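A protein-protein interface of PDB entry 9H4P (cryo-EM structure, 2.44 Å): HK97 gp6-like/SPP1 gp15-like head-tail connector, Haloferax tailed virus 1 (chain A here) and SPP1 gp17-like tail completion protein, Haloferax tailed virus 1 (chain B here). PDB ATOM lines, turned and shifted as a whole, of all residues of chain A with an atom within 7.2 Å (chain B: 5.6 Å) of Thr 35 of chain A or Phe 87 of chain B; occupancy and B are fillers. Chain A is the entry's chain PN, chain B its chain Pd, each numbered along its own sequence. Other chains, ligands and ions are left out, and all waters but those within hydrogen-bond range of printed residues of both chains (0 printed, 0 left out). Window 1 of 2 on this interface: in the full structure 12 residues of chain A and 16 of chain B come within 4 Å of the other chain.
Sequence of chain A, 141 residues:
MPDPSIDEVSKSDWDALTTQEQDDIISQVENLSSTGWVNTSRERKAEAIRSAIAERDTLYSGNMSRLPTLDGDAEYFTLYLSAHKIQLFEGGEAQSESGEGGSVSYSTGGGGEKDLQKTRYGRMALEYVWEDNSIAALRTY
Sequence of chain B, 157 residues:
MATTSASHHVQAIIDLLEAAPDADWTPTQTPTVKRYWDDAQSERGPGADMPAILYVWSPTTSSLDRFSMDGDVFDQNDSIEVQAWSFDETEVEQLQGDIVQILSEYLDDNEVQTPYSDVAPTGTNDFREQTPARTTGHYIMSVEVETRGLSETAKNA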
ATOM      1  N   GLU A  30      13.025 -13.844 -10.891  1.00  0.00           N
ATOM      2  CA  GLU A  30      12.235 -12.644 -10.647  1.00  0.00           C
ATOM      3  C   GLU A  30      12.085 -11.796 -11.915  1.00  0.00           C
ATOM      4  O   GLU A  30      11.233 -10.909 -11.947  1.00  0.00           O
ATOM      5  CB  GLU A  30      12.847 -11.797  -9.530  1.00  0.00           C
ATOM      6  CG  GLU A  30      12.677 -12.372  -8.138  1.00  0.00           C
ATOM      7  CD  GLU A  30      13.251 -11.500  -7.035  1.00  0.00           C
ATOM      8  OE1 GLU A  30      13.989 -10.549  -7.350  1.00  0.00           O
ATOM      9  OE2 GLU A  30      12.962 -11.776  -5.863  1.00  0.00           O
ATOM     10  N   LEU A  32      10.895 -12.986 -14.605  1.00  0.00           N
ATOM     11  CA  LEU A  32       9.728 -13.548 -15.281  1.00  0.00           C
ATOM     12  C   LEU A  32       8.423 -12.851 -14.873  1.00  0.00           C
ATOM     13  O   LEU A  32       7.366 -13.179 -15.409  1.00  0.00           O
ATOM     14  CB  LEU A  32       9.682 -15.067 -15.050  1.00  0.00           C
ATOM     15  CG  LEU A  32      10.496 -15.944 -16.009  1.00  0.00           C
ATOM     16  CD1 LEU A  32      11.971 -15.567 -16.048  1.00  0.00           C
ATOM     17  CD2 LEU A  32      10.365 -17.408 -15.629  1.00  0.00           C
ATOM     18  N   SER A  33       8.487 -11.884 -13.944  1.00  0.00           N
ATOM     19  CA  SER A  33       7.346 -11.026 -13.659  1.00  0.00           C
ATOM     20  C   SER A  33       7.789  -9.575 -13.505  1.00  0.00           C
ATOM     21  O   SER A  33       8.777  -9.296 -12.829  1.00  0.00           O
ATOM     22  CB  SER A  33       6.582 -11.482 -12.443  1.00  0.00           C
ATOM     23  OG  SER A  33       5.477 -10.626 -12.180  1.00  0.00           O
ATOM     24  N   SER A  34       7.010  -8.668 -14.111  1.00  0.00           N
ATOM     25  CA  SER A  34       7.114  -7.227 -13.925  1.00  0.00           C
ATOM     26  C   SER A  34       6.985  -6.834 -12.452  1.00  0.00           C
ATOM     27  O   SER A  34       7.591  -5.852 -12.033  1.00  0.00           O
ATOM     28  CB  SER A  34       6.099  -6.494 -14.764  1.00  0.00           C
ATOM     29  OG  SER A  34       4.774  -6.798 -14.352  1.00  0.00           O
ATOM     30  N   THR A  35       6.193  -7.593 -11.679  1.00  0.00           N
ATOM     31  CA  THR A  35       5.990  -7.343 -10.257  1.00  0.00           C
ATOM     32  C   THR A  35       7.092  -7.980  -9.403  1.00  0.00           C
ATOM     33  O   THR A  35       7.194  -7.672  -8.217  1.00  0.00           O
ATOM     34  CB  THR A  35       4.605  -7.808  -9.781  1.00  0.00           C
ATOM     35  OG1 THR A  35       4.482  -9.217  -9.971  1.00  0.00           O
ATOM     36  CG2 THR A  35       3.455  -7.099 -10.462  1.00  0.00           C
ATOM     37  N   GLY A  36       7.875  -8.899  -9.987  1.00  0.00           N
ATOM     38  CA  GLY A  36       9.049  -9.502  -9.366  1.00  0.00           C
ATOM     39  C   GLY A  36       8.773 -10.362  -8.128  1.00  0.00           C
ATOM     40  O   GLY A  36       9.715 -10.938  -7.584  1.00  0.00           O
ATOM     41  N   TRP A  37       7.501 -10.449  -7.698  1.00  0.00           N
ATOM     42  CA  TRP A  37       7.080 -11.096  -6.458  1.00  0.00           C
ATOM     43  C   TRP A  37       7.846 -10.525  -5.259  1.00  0.00           C
ATOM     44  O   TRP A  37       8.312 -11.274  -4.402  1.00  0.00           O
ATOM     45  CB  TRP A  37       7.162 -12.631  -6.564  1.00  0.00           C
ATOM     46  CG  TRP A  37       6.451 -13.209  -7.751  1.00  0.00           C
ATOM     47  CD1 TRP A  37       5.103 -13.361  -7.903  1.00  0.00           C
ATOM     48  CD2 TRP A  37       7.045 -13.704  -8.968  1.00  0.00           C
ATOM     49  NE1 TRP A  37       4.821 -13.916  -9.123  1.00  0.00           N
ATOM     50  CE2 TRP A  37       5.991 -14.143  -9.799  1.00  0.00           C
ATOM     51  CE3 TRP A  37       8.360 -13.825  -9.441  1.00  0.00           C
ATOM     52  CZ2 TRP A  37       6.217 -14.694 -11.064  1.00  0.00           C
ATOM     53  CZ3 TRP A  37       8.583 -14.365 -10.692  1.00  0.00           C
ATOM     54  CH2 TRP A  37       7.524 -14.792 -11.494  1.00  0.00           C
ATOM     55  N   VAL A  38       7.943  -9.188  -5.200  1.00  0.00           N
ATOM     56  CA  VAL A  38       8.823  -8.466  -4.283  1.00  0.00           C
ATOM     57  C   VAL A  38       8.308  -8.497  -2.841  1.00  0.00           C
ATOM     58  O   VAL A  38       9.103  -8.357  -1.912  1.00  0.00           O
ATOM     59  CB  VAL A  38       9.128  -7.024  -4.746  1.00  0.00           C
ATOM     60  CG1 VAL A  38       9.999  -6.995  -5.992  1.00  0.00           C
ATOM     61  CG2 VAL A  38       7.879  -6.178  -4.938  1.00  0.00           C
ATOM     62  N   ASN A  39       6.991  -8.675  -2.657  1.00  0.00           N
ATOM     63  CA  ASN A  39       6.372  -8.725  -1.337  1.00  0.00           C
ATOM     64  C   ASN A  39       6.506 -10.116  -0.706  1.00  0.00           C
ATOM     65  O   ASN A  39       6.428 -10.242   0.515  1.00  0.00           O
ATOM     66  CB  ASN A  39       4.922  -8.234  -1.370  1.00  0.00           C
ATOM     67  CG  ASN A  39       4.792  -6.824  -1.903  1.00  0.00           C
ATOM     68  OD1 ASN A  39       4.442  -6.621  -3.061  1.00  0.00           O
ATOM     69  ND2 ASN A  39       5.084  -5.843  -1.069  1.00  0.00           N
ATOM     70  N   GLN A  87       3.890 -18.247  -8.254  1.00  0.00           N
ATOM     71  CA  GLN A  87       2.564 -17.700  -8.504  1.00  0.00           C
ATOM     72  C   GLN A  87       1.490 -18.460  -7.721  1.00  0.00           C
ATOM     73  O   GLN A  87       0.551 -17.836  -7.227  1.00  0.00           O
ATOM     74  CB  GLN A  87       2.265 -17.602 -10.004  1.00  0.00           C
ATOM     75  CG  GLN A  87       1.052 -16.734 -10.331  1.00  0.00           C
ATOM     76  CD  GLN A  87       1.195 -15.288  -9.915  1.00  0.00           C
ATOM     77  OE1 GLN A  87       2.246 -14.678 -10.079  1.00  0.00           O
ATOM     78  NE2 GLN A  87       0.127 -14.718  -9.386  1.00  0.00           N
ATOM     79  N   GLU A  90       1.442 -17.406  -4.103  1.00  0.00           N
ATOM     80  CA  GLU A  90       0.664 -16.176  -3.971  1.00  0.00           C
ATOM     81  C   GLU A  90      -0.821 -16.371  -4.321  1.00  0.00           C
ATOM     82  O   GLU A  90      -1.553 -15.386  -4.430  1.00  0.00           O
ATOM     83  CB  GLU A  90       1.279 -15.050  -4.810  1.00  0.00           C
ATOM     84  CG  GLU A  90       2.637 -14.567  -4.323  1.00  0.00           C
ATOM     85  CD  GLU A  90       3.016 -13.148  -4.713  1.00  0.00           C
ATOM     86  OE1 GLU A  90       2.360 -12.570  -5.597  1.00  0.00           O
ATOM     87  OE2 GLU A  90       3.973 -12.623  -4.129  1.00  0.00           O
ATOM     88  N   ARG A 120      -0.075 -18.942 -16.347  1.00  0.00           N
ATOM     89  CA  ARG A 120       0.611 -18.543 -17.575  1.00  0.00           C
ATOM     90  C   ARG A 120       2.008 -19.163 -17.662  1.00  0.00           C
ATOM     91  O   ARG A 120       2.410 -19.614 -18.734  1.00  0.00           O
ATOM     92  CB  ARG A 120       0.609 -17.015 -17.722  1.00  0.00           C
ATOM     93  CG  ARG A 120       1.336 -16.264 -16.614  1.00  0.00           C
ATOM     94  CD  ARG A 120       0.713 -14.925 -16.276  1.00  0.00           C
ATOM     95  NE  ARG A 120       1.591 -14.146 -15.408  1.00  0.00           N
ATOM     96  CZ  ARG A 120       1.291 -13.662 -14.203  1.00  0.00           C
ATOM     97  NH1 ARG A 120       2.203 -12.977 -13.535  1.00  0.00           N
ATOM     98  NH2 ARG A 120       0.095 -13.844 -13.671  1.00  0.00           N
ATOM     99  N   TYR A 121       2.720 -19.199 -16.527  1.00  0.00           N
ATOM    100  CA  TYR A 121       4.040 -19.804 -16.420  1.00  0.00           C
ATOM    101  C   TYR A 121       3.957 -21.319 -16.585  1.00  0.00           C
ATOM    102  O   TYR A 121       4.852 -21.918 -17.179  1.00  0.00           O
ATOM    103  CB  TYR A 121       4.707 -19.397 -15.105  1.00  0.00           C
ATOM    104  CG  TYR A 121       4.765 -17.905 -14.918  1.00  0.00           C
ATOM    105  CD1 TYR A 121       5.525 -17.125 -15.776  1.00  0.00           C
ATOM    106  CD2 TYR A 121       4.038 -17.269 -13.922  1.00  0.00           C
ATOM    107  CE1 TYR A 121       5.575 -15.749 -15.644  1.00  0.00           C
ATOM    108  CE2 TYR A 121       4.085 -15.892 -13.772  1.00  0.00           C
ATOM    109  CZ  TYR A 121       4.856 -15.132 -14.636  1.00  0.00           C
ATOM    110  OH  TYR A 121       4.903 -13.777 -14.492  1.00  0.00           O
ATOM    111  N   PRO B  46       4.459   1.184 -11.036  1.00  0.00           N
ATOM    112  CA  PRO B  46       5.793   0.741 -11.455  1.00  0.00           C
ATOM    113  C   PRO B  46       5.919  -0.779 -11.523  1.00  0.00           C
ATOM    114  O   PRO B  46       5.161  -1.499 -10.879  1.00  0.00           O
ATOM    115  CB  PRO B  46       6.706   1.280 -10.340  1.00  0.00           C
ATOM    116  CG  PRO B  46       5.814   1.341  -9.118  1.00  0.00           C
ATOM    117  CD  PRO B  46       4.455   1.723  -9.664  1.00  0.00           C
ATOM    118  N   GLY B  47       6.873  -1.255 -12.330  1.00  0.00           N
ATOM    119  CA  GLY B  47       7.392  -2.605 -12.180  1.00  0.00           C
ATOM    120  C   GLY B  47       8.466  -2.641 -11.095  1.00  0.00           C
ATOM    121  O   GLY B  47       8.878  -1.594 -10.599  1.00  0.00           O
ATOM    122  N   ALA B  48       8.904  -3.851 -10.726  1.00  0.00           N
ATOM    123  CA  ALA B  48      10.007  -4.042  -9.795  1.00  0.00           C
ATOM    124  C   ALA B  48      11.303  -3.511 -10.412  1.00  0.00           C
ATOM    125  O   ALA B  48      11.439  -3.498 -11.637  1.00  0.00           O
ATOM    126  CB  ALA B  48      10.129  -5.504  -9.436  1.00  0.00           C
ATOM    127  N   TRP B  85       2.024   5.300  -6.446  1.00  0.00           N
ATOM    128  CA  TRP B  85       1.961   3.846  -6.600  1.00  0.00           C
ATOM    129  C   TRP B  85       3.346   3.229  -6.375  1.00  0.00           C
ATOM    130  O   TRP B  85       4.316   3.672  -6.991  1.00  0.00           O
ATOM    131  CB  TRP B  85       1.433   3.453  -7.996  1.00  0.00           C
ATOM    132  CG  TRP B  85      -0.004   3.734  -8.342  1.00  0.00           C
ATOM    133  CD1 TRP B  85      -0.668   4.923  -8.237  1.00  0.00           C
ATOM    134  CD2 TRP B  85      -0.942   2.819  -8.955  1.00  0.00           C
ATOM    135  NE1 TRP B  85      -1.952   4.800  -8.702  1.00  0.00           N
ATOM    136  CE2 TRP B  85      -2.152   3.521  -9.157  1.00  0.00           C
ATOM    137  CE3 TRP B  85      -0.892   1.471  -9.345  1.00  0.00           C
ATOM    138  CZ2 TRP B  85      -3.284   2.916  -9.718  1.00  0.00           C
ATOM    139  CZ3 TRP B  85      -2.007   0.875  -9.904  1.00  0.00           C
ATOM    140  CH2 TRP B  85      -3.193   1.588 -10.086  1.00  0.00           C
ATOM    141  N   SER B  86       3.431   2.204  -5.502  1.00  0.00           N
ATOM    142  CA  SER B  86       4.626   1.389  -5.284  1.00  0.00           C
ATOM    143  C   SER B  86       4.250   0.048  -4.649  1.00  0.00           C
ATOM    144  O   SER B  86       3.163  -0.079  -4.086  1.00  0.00           O
ATOM    145  CB  SER B  86       5.656   2.123  -4.444  1.00  0.00           C
ATOM    146  OG  SER B  86       6.846   1.356  -4.296  1.00  0.00           O
ATOM    147  N   PHE B  87       5.164  -0.938  -4.712  1.00  0.00           N
ATOM    148  CA  PHE B  87       5.023  -2.213  -4.015  1.00  0.00           C
ATOM    149  C   PHE B  87       5.403  -2.117  -2.534  1.00  0.00           C
ATOM    150  O   PHE B  87       5.146  -3.056  -1.780  1.00  0.00           O
ATOM    151  CB  PHE B  87       5.866  -3.300  -4.687  1.00  0.00           C
ATOM    152  CG  PHE B  87       5.498  -3.577  -6.121  1.00  0.00           C
ATOM    153  CD1 PHE B  87       4.318  -4.239  -6.431  1.00  0.00           C
ATOM    154  CD2 PHE B  87       6.320  -3.162  -7.159  1.00  0.00           C
ATOM    155  CE1 PHE B  87       3.968  -4.484  -7.750  1.00  0.00           C
ATOM    156  CE2 PHE B  87       5.970  -3.409  -8.479  1.00  0.00           C
ATOM    157  CZ  PHE B  87       4.797  -4.072  -8.771  1.00  0.00           C
ATOM    158  N   ASP B  88       6.014  -0.997  -2.120  1.00  0.00           N
ATOM    159  CA  ASP B  88       6.488  -0.797  -0.757  1.00  0.00           C
ATOM    160  C   ASP B  88       5.500   0.089   0.005  1.00  0.00           C
ATOM    161  O   ASP B  88       5.345   1.268  -0.315  1.00  0.00           O
ATOM    162  CB  ASP B  88       7.931  -0.269  -0.770  1.00  0.00           C
ATOM    163  CG  ASP B  88       8.559   0.043   0.580  1.00  0.00           C
ATOM    164  OD1 ASP B  88       7.840   0.060   1.592  1.00  0.00           O
ATOM    165  OD2 ASP B  88       9.782   0.260   0.606  1.00  0.00           O
ATOM    166  N   GLU B  89       4.872  -0.489   1.042  1.00  0.00           N
ATOM    167  CA  GLU B  89       3.847   0.142   1.871  1.00  0.00           C
ATOM    168  C   GLU B  89       4.383   1.338   2.667  1.00  0.00           C
ATOM    169  O   GLU B  89       3.592   2.149   3.149  1.00  0.00           O
ATOM    170  CB  GLU B  89       3.227  -0.891   2.817  1.00  0.00           C
ATOM    171  CG  GLU B  89       4.225  -1.534   3.768  1.00  0.00           C
ATOM    172  CD  GLU B  89       3.644  -2.543   4.735  1.00  0.00           C
ATOM    173  OE1 GLU B  89       2.672  -2.209   5.422  1.00  0.00           O
ATOM    174  OE2 GLU B  89       4.175  -3.660   4.800  1.00  0.00           O
ATOM    175  N   GLU B  91       7.157   3.179   1.262  1.00  0.00           N
ATOM    176  CA  GLU B  91       7.571   4.112   0.224  1.00  0.00           C
ATOM    177  C   GLU B  91       6.409   5.028  -0.164  1.00  0.00           C
ATOM    178  O   GLU B  91       6.622   6.230  -0.315  1.00  0.00           O
ATOM    179  CB  GLU B  91       8.150   3.391  -0.993  1.00  0.00           C
ATOM    180  CG  GLU B  91       8.816   4.325  -1.985  1.00  0.00           C
ATOM    181  CD  GLU B  91       9.479   3.615  -3.147  1.00  0.00           C
ATOM    182  OE1 GLU B  91       8.850   2.723  -3.731  1.00  0.00           O
ATOM    183  OE2 GLU B  91      10.630   3.954  -3.459  1.00  0.00           O
ATOM    184  N   THR B 136       1.714  -9.951  -4.605  1.00  0.00           N
ATOM    185  CA  THR B 136       2.392  -8.687  -4.852  1.00  0.00           C
ATOM    186  C   THR B 136       1.477  -7.836  -5.732  1.00  0.00           C
ATOM    187  O   THR B 136       0.861  -8.334  -6.673  1.00  0.00           O
ATOM    188  CB  THR B 136       3.803  -8.866  -5.435  1.00  0.00           C
ATOM    189  OG1 THR B 136       4.430  -7.587  -5.536  1.00  0.00           O
ATOM    190  CG2 THR B 136       3.814  -9.527  -6.794  1.00  0.00           C
ATOM    191  N   GLY B 137       1.389  -6.552  -5.397  1.00  0.00           N
ATOM    192  CA  GLY B 137       0.491  -5.609  -6.039  1.00  0.00           C
ATOM    193  C   GLY B 137       0.656  -4.257  -5.363  1.00  0.00           C
ATOM    194  O   GLY B 137       1.102  -4.197  -4.217  1.00  0.00           O
ATOM    195  N   HIS B 138       0.304  -3.183  -6.075  1.00  0.00           N
ATOM    196  CA  HIS B 138       0.632  -1.837  -5.631  1.00  0.00           C
ATOM    197  C   HIS B 138      -0.152  -1.455  -4.384  1.00  0.00           C
ATOM    198  O   HIS B 138      -1.357  -1.691  -4.296  1.00  0.00           O
ATOM    199  CB  HIS B 138       0.409  -0.832  -6.763  1.00  0.00           C
ATOM    200  CG  HIS B 138       1.207  -1.191  -7.963  1.00  0.00           C
ATOM    201  ND1 HIS B 138       0.696  -1.951  -8.997  1.00  0.00           N
ATOM    202  CD2 HIS B 138       2.501  -0.961  -8.261  1.00  0.00           C
ATOM    203  CE1 HIS B 138       1.634  -2.143  -9.899  1.00  0.00           C
ATOM    204  NE2 HIS B 138       2.746  -1.543  -9.471  1.00  0.00           N
ATOM    205  N   TYR B 139       0.570  -0.856  -3.433  1.00  0.00           N
ATOM    206  CA  TYR B 139      -0.016   0.018  -2.432  1.00  0.00           C
ATOM    207  C   TYR B 139      -0.257   1.380  -3.076  1.00  0.00           C
ATOM    208  O   TYR B 139       0.544   1.821  -3.901  1.00  0.00           O
ATOM    209  CB  TYR B 139       0.898   0.095  -1.205  1.00  0.00           C
ATOM    210  CG  TYR B 139       1.023  -1.235  -0.507  1.00  0.00           C
ATOM    211  CD1 TYR B 139       0.002  -1.693   0.314  1.00  0.00           C
ATOM    212  CD2 TYR B 139       2.116  -2.068  -0.716  1.00  0.00           C
ATOM    213  CE1 TYR B 139       0.073  -2.929   0.934  1.00  0.00           C
ATOM    214  CE2 TYR B 139       2.202  -3.308  -0.103  1.00  0.00           C
ATOM    215  CZ  TYR B 139       1.178  -3.738   0.725  1.00  0.00           C
ATOM    216  OH  TYR B 139       1.257  -4.953   1.340  1.00  0.00           O
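Phe 87 of chain B touches just these residues of chain A: Thr 35 (3.7 Å), Val 38 (3.5 Å) and Asn 39 (2.9 Å).
Of the printed residues of chain A, Gly 47 of chain B touches Ser 34.
Of the printed residues of chain B, Ser 34 of chain A touches Gly 47 and Ala 48.
Glu 89 of chain B touches none of the printed residues of chain A.
Trp 85 of chain B touches none of the printed residues of chain A.
The nearest residue of chain A that does not touch Phe 87 of chain B is Ser 34 of chain A (4.6 Å).
The nearest printed residue of chain A that does not touch Thr 136 of chain B is Gly 36 of chain A (5.2 Å).
The backbone carbonyl oxygen of Ser 34 of chain A sits at hydrogen-bond distance from the backbone NH of Ala 48 of chain B (2.7 Å).
The backbone carbonyl oxygen (O) of Phe 87 of chain B sits at hydrogen-bond distance from the side-chain amide nitrogen (ND2) of Asn 39 of chain A (2.9 Å).
The side-chain hydroxyl (OG1) of Thr 136 of chain B sits at hydrogen-bond distance from the side-chain amide oxygen (OD1) of Asn 39 of chain A, 2.7 Å away.
N of Thr 136 of chain B sits at hydrogen-bond distance from OE1 of Glu 90 of chain A (2.9 Å).
Of the 13 printed residues of chain B, 6 touch a printed residue of chain A.
Printed residues of chain B that touch a printed residue of chain A: Gly 47, Ala 48, Phe 87, Thr 136, Gly 137 and Tyr 139.
Of the 13 printed residues of chain A, 6 touch a printed residue of chain B.
Printed residues of chain A that touch a printed residue of chain B: Ser 34, Thr 35, Trp 37, Val 38, Asn 39 and Glu 90.
Hydrophobic or aromatic side chains of chain A within 4 Å of the printed part of chain B: Val 38.
Among the printed residues, 14 pairs touch across the chains.
The backbone carbonyl oxygen (O) of Ser 86 of chain B sits at hydrogen-bond distance from the backbone NH (N) of Tyr 139 of chain B, at 2.8 Å.
The side-chain hydroxyl of Ser 33 of chain A is in hydrogen-bond range of the side-chain hydroxyl of Thr 35 of chain A (2.8 Å).
The indole nitrogen (NE1) of Trp 37 of chain A lies within hydrogen-bond range of the side-chain amide oxygen (OE1) of Gln 87 of chain A, at 2.9 Å.
Among the printed residues, merely in contact across the chains: Ser 34 of chain A with Gly 47 of chain B (3.3 Å), Thr 35 of chain A with Thr 136 of chain B (3.3 Å), Val 38 of chain A with Phe 87 of chain B (3.5 Å), Trp 37 of chain A with Thr 136 of chain B (3.6 Å), Thr 35 of chain A with Phe 87 of chain B (3.7 Å), Val 38 of chain A with Ala 48 of chain B (3.8 Å), Val 38 of chain A with Thr 136 of chain B (3.8 Å), Asn 39 of chain A with Gly 137 of chain B (3.8 Å), Thr 35 of chain A with Ala 48 of chain B (3.8 Å) and Asn 39 of chain A with Tyr 139 of chain B (3.96 Å).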
